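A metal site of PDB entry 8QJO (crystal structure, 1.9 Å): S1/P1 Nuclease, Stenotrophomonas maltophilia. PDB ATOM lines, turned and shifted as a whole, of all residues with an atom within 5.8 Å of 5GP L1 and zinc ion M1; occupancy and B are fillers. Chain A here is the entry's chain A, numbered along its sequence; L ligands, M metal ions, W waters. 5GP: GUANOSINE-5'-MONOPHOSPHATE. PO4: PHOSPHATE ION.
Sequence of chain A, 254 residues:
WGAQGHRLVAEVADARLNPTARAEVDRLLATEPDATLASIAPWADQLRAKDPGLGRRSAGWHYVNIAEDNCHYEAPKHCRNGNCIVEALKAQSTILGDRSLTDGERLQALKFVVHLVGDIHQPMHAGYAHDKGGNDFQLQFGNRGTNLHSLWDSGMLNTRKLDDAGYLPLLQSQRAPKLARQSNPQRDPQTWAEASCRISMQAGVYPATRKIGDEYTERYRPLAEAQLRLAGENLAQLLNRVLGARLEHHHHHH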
ATOM      1  N   TRP A   1      25.403  -1.824 -11.955  1.00  0.00           N
ATOM      2  CA  TRP A   1      26.565  -2.623 -11.523  1.00  0.00           C
ATOM      3  C   TRP A   1      27.673  -1.702 -10.988  1.00  0.00           C
ATOM      4  O   TRP A   1      27.710  -0.544 -11.379  1.00  0.00           O
ATOM      5  CB  TRP A   1      27.119  -3.519 -12.661  1.00  0.00           C
ATOM      6  CG  TRP A   1      26.083  -4.294 -13.397  1.00  0.00           C
ATOM      7  CD1 TRP A   1      25.544  -4.006 -14.617  1.00  0.00           C
ATOM      8  CD2 TRP A   1      25.401  -5.479 -12.936  1.00  0.00           C
ATOM      9  NE1 TRP A   1      24.572  -4.913 -14.935  1.00  0.00           N
ATOM     10  CE2 TRP A   1      24.479  -5.855 -13.931  1.00  0.00           C
ATOM     11  CE3 TRP A   1      25.517  -6.272 -11.792  1.00  0.00           C
ATOM     12  CZ2 TRP A   1      23.646  -6.952 -13.816  1.00  0.00           C
ATOM     13  CZ3 TRP A   1      24.704  -7.380 -11.674  1.00  0.00           C
ATOM     14  CH2 TRP A   1      23.776  -7.711 -12.667  1.00  0.00           C
ATOM     15  N   ASP A  45      29.364   6.601 -14.178  1.00  0.00           N
ATOM     16  CA  ASP A  45      29.283   6.601 -12.682  1.00  0.00           C
ATOM     17  C   ASP A  45      30.313   7.586 -12.110  1.00  0.00           C
ATOM     18  O   ASP A  45      29.985   8.230 -11.114  1.00  0.00           O
ATOM     19  CB  ASP A  45      29.504   5.226 -12.050  1.00  0.00           C
ATOM     20  CG  ASP A  45      28.360   4.258 -12.255  1.00  0.00           C
ATOM     21  OD1 ASP A  45      27.198   4.733 -12.515  1.00  0.00           O
ATOM     22  OD2 ASP A  45      28.639   3.040 -12.161  1.00  0.00           O
ATOM     23  N   ARG A  48      28.854  11.015 -12.847  1.00  0.00           N
ATOM     24  CA  ARG A  48      27.809  11.255 -11.817  1.00  0.00           C
ATOM     25  C   ARG A  48      28.457  11.737 -10.509  1.00  0.00           C
ATOM     26  O   ARG A  48      27.927  12.648  -9.889  1.00  0.00           O
ATOM     27  CB  ARG A  48      26.989   9.994 -11.513  1.00  0.00           C
ATOM     28  CG  ARG A  48      25.832  10.252 -10.563  1.00  0.00           C
ATOM     29  CD  ARG A  48      25.051   9.011 -10.169  1.00  0.00           C
ATOM     30  NE  ARG A  48      25.947   7.947  -9.711  1.00  0.00           N
ATOM     31  CZ  ARG A  48      25.800   6.654  -9.942  1.00  0.00           C
ATOM     32  NH1 ARG A  48      24.751   6.152 -10.621  1.00  0.00           N
ATOM     33  NH2 ARG A  48      26.724   5.835  -9.460  1.00  0.00           N
ATOM     34  N   ALA A  59      22.108  11.708 -13.438  1.00  0.00           N
ATOM     35  CA  ALA A  59      22.019  10.713 -12.345  1.00  0.00           C
ATOM     36  C   ALA A  59      20.797   9.824 -12.558  1.00  0.00           C
ATOM     37  O   ALA A  59      20.936   8.599 -12.450  1.00  0.00           O
ATOM     38  CB  ALA A  59      21.955  11.355 -10.969  1.00  0.00           C
ATOM     39  N   HIS A  62      20.431   6.403 -14.912  1.00  0.00           N
ATOM     40  CA  HIS A  62      20.982   5.056 -14.550  1.00  0.00           C
ATOM     41  C   HIS A  62      19.877   4.072 -14.214  1.00  0.00           C
ATOM     42  O   HIS A  62      20.154   2.853 -14.181  1.00  0.00           O
ATOM     43  CB  HIS A  62      22.033   5.163 -13.434  1.00  0.00           C
ATOM     44  CG  HIS A  62      23.246   5.945 -13.865  1.00  0.00           C
ATOM     45  ND1 HIS A  62      24.503   5.416 -13.906  1.00  0.00           N
ATOM     46  CD2 HIS A  62      23.358   7.222 -14.291  1.00  0.00           C
ATOM     47  CE1 HIS A  62      25.343   6.337 -14.317  1.00  0.00           C
ATOM     48  NE2 HIS A  62      24.671   7.463 -14.560  1.00  0.00           N
ATOM     49  N   TYR A  63      18.651   4.535 -13.989  1.00  0.00           N
ATOM     50  CA  TYR A  63      17.581   3.677 -13.448  1.00  0.00           C
ATOM     51  C   TYR A  63      16.211   4.137 -13.929  1.00  0.00           C
ATOM     52  O   TYR A  63      16.050   5.173 -14.617  1.00  0.00           O
ATOM     53  CB  TYR A  63      17.688   3.618 -11.912  1.00  0.00           C
ATOM     54  CG  TYR A  63      17.489   4.952 -11.249  1.00  0.00           C
ATOM     55  CD1 TYR A  63      16.213   5.454 -11.023  1.00  0.00           C
ATOM     56  CD2 TYR A  63      18.573   5.735 -10.896  1.00  0.00           C
ATOM     57  CE1 TYR A  63      16.017   6.691 -10.426  1.00  0.00           C
ATOM     58  CE2 TYR A  63      18.386   6.976 -10.310  1.00  0.00           C
ATOM     59  CZ  TYR A  63      17.103   7.452 -10.070  1.00  0.00           C
ATOM     60  OH  TYR A  63      16.937   8.679  -9.500  1.00  0.00           O
ATOM     61  N   VAL A  64      15.209   3.321 -13.604  1.00  0.00           N
ATOM     62  CA  VAL A  64      13.786   3.671 -13.767  1.00  0.00           C
ATOM     63  C   VAL A  64      12.969   2.887 -12.727  1.00  0.00           C
ATOM     64  O   VAL A  64      13.187   1.675 -12.576  1.00  0.00           O
ATOM     65  CB  VAL A  64      13.327   3.418 -15.202  1.00  0.00           C
ATOM     66  CG1 VAL A  64      13.215   1.941 -15.556  1.00  0.00           C
ATOM     67  CG2 VAL A  64      12.014   4.131 -15.477  1.00  0.00           C
ATOM     68  N   ASN A  65      12.051   3.555 -12.040  1.00  0.00           N
ATOM     69  CA  ASN A  65      11.275   2.948 -10.934  1.00  0.00           C
ATOM     70  C   ASN A  65       9.915   2.536 -11.502  1.00  0.00           C
ATOM     71  O   ASN A  65       9.109   3.415 -11.714  1.00  0.00           O
ATOM     72  CB  ASN A  65      11.128   3.892  -9.742  1.00  0.00           C
ATOM     73  CG  ASN A  65      12.459   4.244  -9.125  1.00  0.00           C
ATOM     74  OD1 ASN A  65      13.309   3.368  -8.931  1.00  0.00           O
ATOM     75  ND2 ASN A  65      12.651   5.513  -8.796  1.00  0.00           N
ATOM     76  N   ASP A 119      23.563  -1.223 -16.884  1.00  0.00           N
ATOM     77  CA  ASP A 119      22.638  -0.852 -15.797  1.00  0.00           C
ATOM     78  C   ASP A 119      21.220  -1.336 -16.083  1.00  0.00           C
ATOM     79  O   ASP A 119      20.580  -1.747 -15.152  1.00  0.00           O
ATOM     80  CB  ASP A 119      22.641   0.653 -15.545  1.00  0.00           C
ATOM     81  CG  ASP A 119      23.752   1.105 -14.581  1.00  0.00           C
ATOM     82  OD1 ASP A 119      24.483   0.234 -14.061  1.00  0.00           O
ATOM     83  OD2 ASP A 119      23.857   2.315 -14.369  1.00  0.00           O
ATOM     84  N   GLN A 122      20.571  -4.681 -14.685  1.00  0.00           N
ATOM     85  CA  GLN A 122      20.694  -4.892 -13.226  1.00  0.00           C
ATOM     86  C   GLN A 122      19.272  -4.810 -12.678  1.00  0.00           C
ATOM     87  O   GLN A 122      18.631  -3.753 -12.757  1.00  0.00           O
ATOM     88  CB  GLN A 122      21.689  -3.891 -12.638  1.00  0.00           C
ATOM     89  CG  GLN A 122      22.449  -4.341 -11.391  1.00  0.00           C
ATOM     90  CD  GLN A 122      21.606  -4.326 -10.142  1.00  0.00           C
ATOM     91  OE1 GLN A 122      20.619  -5.040 -10.044  1.00  0.00           O
ATOM     92  NE2 GLN A 122      21.978  -3.484  -9.168  1.00  0.00           N
ATOM     93  N   MET A 124      17.767  -4.311  -9.879  1.00  0.00           N
ATOM     94  CA  MET A 124      17.454  -3.265  -8.894  1.00  0.00           C
ATOM     95  C   MET A 124      17.441  -1.877  -9.568  1.00  0.00           C
ATOM     96  O   MET A 124      16.863  -0.936  -9.007  1.00  0.00           O
ATOM     97  CB  MET A 124      18.430  -3.309  -7.719  1.00  0.00           C
ATOM     98  CG  MET A 124      18.424  -4.668  -7.020  1.00  0.00           C
ATOM     99  SD  MET A 124      16.777  -5.285  -6.477  1.00  0.00           S
ATOM    100  CE  MET A 124      16.320  -3.949  -5.393  1.00  0.00           C
ATOM    101  N   HIS A 125      18.009  -1.752 -10.762  1.00  0.00           N
ATOM    102  CA  HIS A 125      17.953  -0.507 -11.578  1.00  0.00           C
ATOM    103  C   HIS A 125      16.558  -0.306 -12.223  1.00  0.00           C
ATOM    104  O   HIS A 125      16.339   0.726 -12.914  1.00  0.00           O
ATOM    105  CB  HIS A 125      19.107  -0.514 -12.557  1.00  0.00           C
ATOM    106  CG  HIS A 125      20.392  -0.060 -11.949  1.00  0.00           C
ATOM    107  ND1 HIS A 125      21.055   1.066 -12.393  1.00  0.00           N
ATOM    108  CD2 HIS A 125      21.176  -0.583 -10.973  1.00  0.00           C
ATOM    109  CE1 HIS A 125      22.157   1.227 -11.688  1.00  0.00           C
ATOM    110  NE2 HIS A 125      22.255   0.244 -10.820  1.00  0.00           N
ATOM    111  N   ALA A 126      15.620  -1.244 -12.058  1.00  0.00           N
ATOM    112  CA  ALA A 126      14.253  -1.132 -12.627  1.00  0.00           C
ATOM    113  C   ALA A 126      13.220  -1.454 -11.549  1.00  0.00           C
ATOM    114  O   ALA A 126      12.087  -1.793 -11.913  1.00  0.00           O
ATOM    115  CB  ALA A 126      14.107  -2.020 -13.824  1.00  0.00           C
ATOM    116  N   GLY A 127      13.584  -1.323 -10.272  1.00  0.00           N
ATOM    117  CA  GLY A 127      12.789  -1.757  -9.103  1.00  0.00           C
ATOM    118  C   GLY A 127      11.879  -0.667  -8.553  1.00  0.00           C
ATOM    119  O   GLY A 127      11.225   0.037  -9.317  1.00  0.00           O
ATOM    120  N   TYR A 128      11.807  -0.568  -7.214  1.00  0.00           N
ATOM    121  CA  TYR A 128      10.842   0.296  -6.490  1.00  0.00           C
ATOM    122  C   TYR A 128      11.408   1.703  -6.273  1.00  0.00           C
ATOM    123  O   TYR A 128      12.578   1.866  -5.869  1.00  0.00           O
ATOM    124  CB  TYR A 128      10.489  -0.326  -5.135  1.00  0.00           C
ATOM    125  CG  TYR A 128       9.658  -1.582  -5.208  1.00  0.00           C
ATOM    126  CD1 TYR A 128       8.272  -1.523  -5.222  1.00  0.00           C
ATOM    127  CD2 TYR A 128      10.254  -2.832  -5.273  1.00  0.00           C
ATOM    128  CE1 TYR A 128       7.488  -2.669  -5.279  1.00  0.00           C
ATOM    129  CE2 TYR A 128       9.490  -3.989  -5.328  1.00  0.00           C
ATOM    130  CZ  TYR A 128       8.108  -3.901  -5.336  1.00  0.00           C
ATOM    131  OH  TYR A 128       7.344  -5.025  -5.416  1.00  0.00           O
ATOM    132  N   ALA A 129      10.588   2.703  -6.575  1.00  0.00           N
ATOM    133  CA  ALA A 129      10.773   4.084  -6.091  1.00  0.00           C
ATOM    134  C   ALA A 129      10.815   4.102  -4.561  1.00  0.00           C
ATOM    135  O   ALA A 129      11.573   4.898  -3.995  1.00  0.00           O
ATOM    136  CB  ALA A 129       9.652   4.939  -6.631  1.00  0.00           C
ATOM    137  N   LYS A 132      14.137   3.240  -3.281  1.00  0.00           N
ATOM    138  CA  LYS A 132      15.147   3.763  -4.260  1.00  0.00           C
ATOM    139  C   LYS A 132      15.977   2.610  -4.845  1.00  0.00           C
ATOM    140  O   LYS A 132      17.195   2.596  -4.695  1.00  0.00           O
ATOM    141  CB  LYS A 132      16.053   4.810  -3.623  1.00  0.00           C
ATOM    142  CG  LYS A 132      15.295   5.935  -2.928  1.00  0.00           C
ATOM    143  CD  LYS A 132      15.981   7.288  -2.980  1.00  0.00           C
ATOM    144  CE  LYS A 132      17.495   7.211  -3.067  1.00  0.00           C
ATOM    145  NZ  LYS A 132      18.154   8.420  -2.490  1.00  0.00           N
ATOM    146  N   GLY A 133      15.338   1.667  -5.513  1.00  0.00           N
ATOM    147  CA  GLY A 133      16.038   0.558  -6.173  1.00  0.00           C
ATOM    148  C   GLY A 133      16.795  -0.317  -5.194  1.00  0.00           C
ATOM    149  O   GLY A 133      17.809  -0.837  -5.595  1.00  0.00           O
ATOM    150  N   GLY A 134      16.351  -0.407  -3.948  1.00  0.00           N
ATOM    151  CA  GLY A 134      16.913  -1.293  -2.907  1.00  0.00           C
ATOM    152  C   GLY A 134      17.973  -0.616  -2.062  1.00  0.00           C
ATOM    153  O   GLY A 134      18.479  -1.270  -1.142  1.00  0.00           O
ATOM    154  N   ASN A 135      18.328   0.634  -2.349  1.00  0.00           N
ATOM    155  CA  ASN A 135      19.325   1.383  -1.540  1.00  0.00           C
ATOM    156  C   ASN A 135      18.858   1.503  -0.084  1.00  0.00           C
ATOM    157  O   ASN A 135      19.697   1.407   0.808  1.00  0.00           O
ATOM    158  CB  ASN A 135      19.633   2.751  -2.132  1.00  0.00           C
ATOM    159  CG  ASN A 135      20.627   2.630  -3.254  1.00  0.00           C
ATOM    160  OD1 ASN A 135      21.766   2.258  -3.022  1.00  0.00           O
ATOM    161  ND2 ASN A 135      20.173   2.866  -4.481  1.00  0.00           N
ATOM    162  N   HIS A 149      20.580  -2.945  -3.055  1.00  0.00           N
ATOM    163  CA  HIS A 149      21.091  -2.371  -4.333  1.00  0.00           C
ATOM    164  C   HIS A 149      22.565  -2.749  -4.497  1.00  0.00           C
ATOM    165  O   HIS A 149      22.922  -3.297  -5.547  1.00  0.00           O
ATOM    166  CB  HIS A 149      20.874  -0.856  -4.450  1.00  0.00           C
ATOM    167  CG  HIS A 149      21.163  -0.371  -5.837  1.00  0.00           C
ATOM    168  ND1 HIS A 149      20.159  -0.215  -6.779  1.00  0.00           N
ATOM    169  CD2 HIS A 149      22.328  -0.065  -6.450  1.00  0.00           C
ATOM    170  CE1 HIS A 149      20.692   0.232  -7.904  1.00  0.00           C
ATOM    171  NE2 HIS A 149      22.028   0.275  -7.756  1.00  0.00           N
ATOM    172  N   ASP A 153      24.626  -4.791  -7.329  1.00  0.00           N
ATOM    173  CA  ASP A 153      25.679  -4.026  -8.039  1.00  0.00           C
ATOM    174  C   ASP A 153      27.008  -4.763  -8.013  1.00  0.00           C
ATOM    175  O   ASP A 153      27.653  -4.848  -9.099  1.00  0.00           O
ATOM    176  CB  ASP A 153      25.855  -2.594  -7.513  1.00  0.00           C
ATOM    177  CG  ASP A 153      24.970  -1.581  -8.206  1.00  0.00           C
ATOM    178  OD1 ASP A 153      24.278  -1.975  -9.227  1.00  0.00           O
ATOM    179  OD2 ASP A 153      25.032  -0.399  -7.799  1.00  0.00           O
HETATM  180  P   5GP L   1      23.395   6.778  -5.351  1.00  0.00           P
HETATM  181  O1P 5GP L   1      24.609   6.868  -6.240  1.00  0.00           O
HETATM  182  O2P 5GP L   1      23.636   6.646  -3.847  1.00  0.00           O
HETATM  183  O3P 5GP L   1      22.359   7.901  -5.644  1.00  0.00           O
HETATM  184  O5' 5GP L   1      22.606   5.365  -5.751  1.00  0.00           O
HETATM  185  C5' 5GP L   1      23.285   4.110  -5.690  1.00  0.00           C
HETATM  186  C4' 5GP L   1      22.774   3.265  -6.823  1.00  0.00           C
HETATM  187  O4' 5GP L   1      21.335   3.228  -6.765  1.00  0.00           O
HETATM  188  C3' 5GP L   1      23.145   3.715  -8.241  1.00  0.00           C
HETATM  189  O3' 5GP L   1      23.472   2.589  -9.051  1.00  0.00           O
HETATM  190  C2' 5GP L   1      21.903   4.505  -8.686  1.00  0.00           C
HETATM  191  O2' 5GP L   1      21.658   4.421 -10.085  1.00  0.00           O
HETATM  192  C1' 5GP L   1      20.779   3.756  -7.962  1.00  0.00           C
HETATM  193  N9  5GP L   1      19.617   4.563  -7.585  1.00  0.00           N
HETATM  194  C8  5GP L   1      19.535   5.780  -6.928  1.00  0.00           C
HETATM  195  N7  5GP L   1      18.291   6.133  -6.636  1.00  0.00           N
HETATM  196  C5  5GP L   1      17.519   5.110  -7.178  1.00  0.00           C
HETATM  197  C6  5GP L   1      16.118   4.985  -7.326  1.00  0.00           C
HETATM  198  O6  5GP L   1      15.270   5.808  -6.985  1.00  0.00           O
HETATM  199  N1  5GP L   1      15.759   3.859  -8.042  1.00  0.00           N
HETATM  200  C2  5GP L   1      16.651   2.923  -8.556  1.00  0.00           C
HETATM  201  N2  5GP L   1      16.116   1.880  -9.224  1.00  0.00           N
HETATM  202  N3  5GP L   1      17.978   3.030  -8.429  1.00  0.00           N
HETATM  203  C4  5GP L   1      18.334   4.123  -7.749  1.00  0.00           C
HETATM  204  P   PO4 L   2      25.527   2.365 -10.940  1.00  0.00           P
HETATM  205  O1  PO4 L   2      26.447   2.961  -9.888  1.00  0.00           O
HETATM  206  O2  PO4 L   2      24.841   1.177 -10.357  1.00  0.00           O
HETATM  207  O3  PO4 L   2      26.368   1.912 -12.151  1.00  0.00           O
HETATM  208  O4  PO4 L   2      24.535   3.375 -11.396  1.00  0.00           O
HETATM  209 ZN    ZN M   1      23.457   0.416  -9.209  1.00  0.00          ZN
HETATM  210 ZN    ZN M   2      26.142   0.088 -12.740  1.00  0.00          ZN
HETATM  211 ZN    ZN M   3      25.308   3.506 -13.482  1.00  0.00          ZN
HETATM  212  O   HOH W   1      21.677   8.559  -8.257  1.00  0.00           O
HETATM  213  O   HOH W   2      25.823   9.026  -2.760  1.00  0.00           O
HETATM  214  O   HOH W   3      22.310   7.330 -10.372  1.00  0.00           O
HETATM  215  O   HOH W   4      25.899   2.438  -7.008  1.00  0.00           O
HETATM  216  O   HOH W   5      14.873   8.540  -7.169  1.00  0.00           O
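ND2 of Asn 135 is in hydrogen-bond range of O4' of 5GP L1 (2.6 Å). The side-chain amide oxygen (OD1) of Asn 65 is in hydrogen-bond range of a nitrogen (N1) of 5GP L1, at 2.7 Å. A nitrogen (N2) of 5GP L1 is in hydrogen-bond range of the backbone carbonyl oxygen of Met 124. The guanidinium group (NE) of Arg 48 is in salt-bridge range of an oxygen (O1P) of 5GP L1 (3.9 Å).
A ring nitrogen (ND1) of His 125 sits at hydrogen-bond distance from the backbone carbonyl oxygen of His 62 (2.7 Å). The backbone carbonyl oxygen (O) of His 125 sits at hydrogen-bond distance from the backbone NH (N) of Val 64 (2.9 Å). The backbone NH (N) of His 149 is in hydrogen-bond range of the backbone carbonyl oxygen (O) of Gly 134. The backbone NH (N) of Asp 153 lies close to the side-chain amide nitrogen (NE2) of Gln 122. The side-chain amide nitrogen (ND2) of Asn 135 sits at hydrogen-bond distance from the backbone carbonyl oxygen (O) of Lys 132 (3.0 Å). The side-chain amide oxygen of Asn 65 lies close to the backbone carbonyl oxygen of Tyr 128, 3.5 Å away. The backbone NH of Met 124 sits at hydrogen-bond distance from the side-chain amide oxygen of Gln 122 (2.9 Å). OD1 of Asp 45 sits close to NH2 of Arg 48, at 3.3 Å.
N of Gly 133 lies close to N1 of 5GP L1 (3.4 Å). CB of His 62 touches O2' of 5GP L1 (3.5 Å). CD1 of Tyr 63 touches N1 of 5GP L1, 3.4 Å away. Lys 132 touches 5GP L1 (CA to O6, 3.4 Å). Hydrophobic or aromatic side chains within 4 Å of 5GP L1: His 62, Tyr 63, His 125 and His 149. Of the 22 residues printed, 11 come within 4 Å of 5GP L1. Along chain A the residues within 4 Å of 5GP L1 span positions 48 to 153. The nearest printed residue that does not touch 5GP L1 is Gly 127 (4.2 Å).
Three residues have an atom within 4 Å of zinc ion M1: His 125, His 149 and Asp 153. The nearest printed residue that does not touch zinc ion M1 is Trp 1 (4.04 Å).
Zinc ion M1 is bound by O2 of PO4 L2, NE2 of His 125, NE2 of His 149, O3' of 5GP L1, OD2 of Asp 153 and OD1 of Asp 153.
Water W5 lies within hydrogen-bond range of an oxygen (O6) of 5GP L1 (2.8 Å) and the side-chain hydroxyl of Tyr 63 (3.1 Å). Water W3 lies within hydrogen-bond range of the guanidinium group (NH1) of Arg 48 (2.7 Å), the backbone carbonyl oxygen (O) of Ala 59 (2.8 Å) and an oxygen (O2') of 5GP L1 (3.0 Å).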
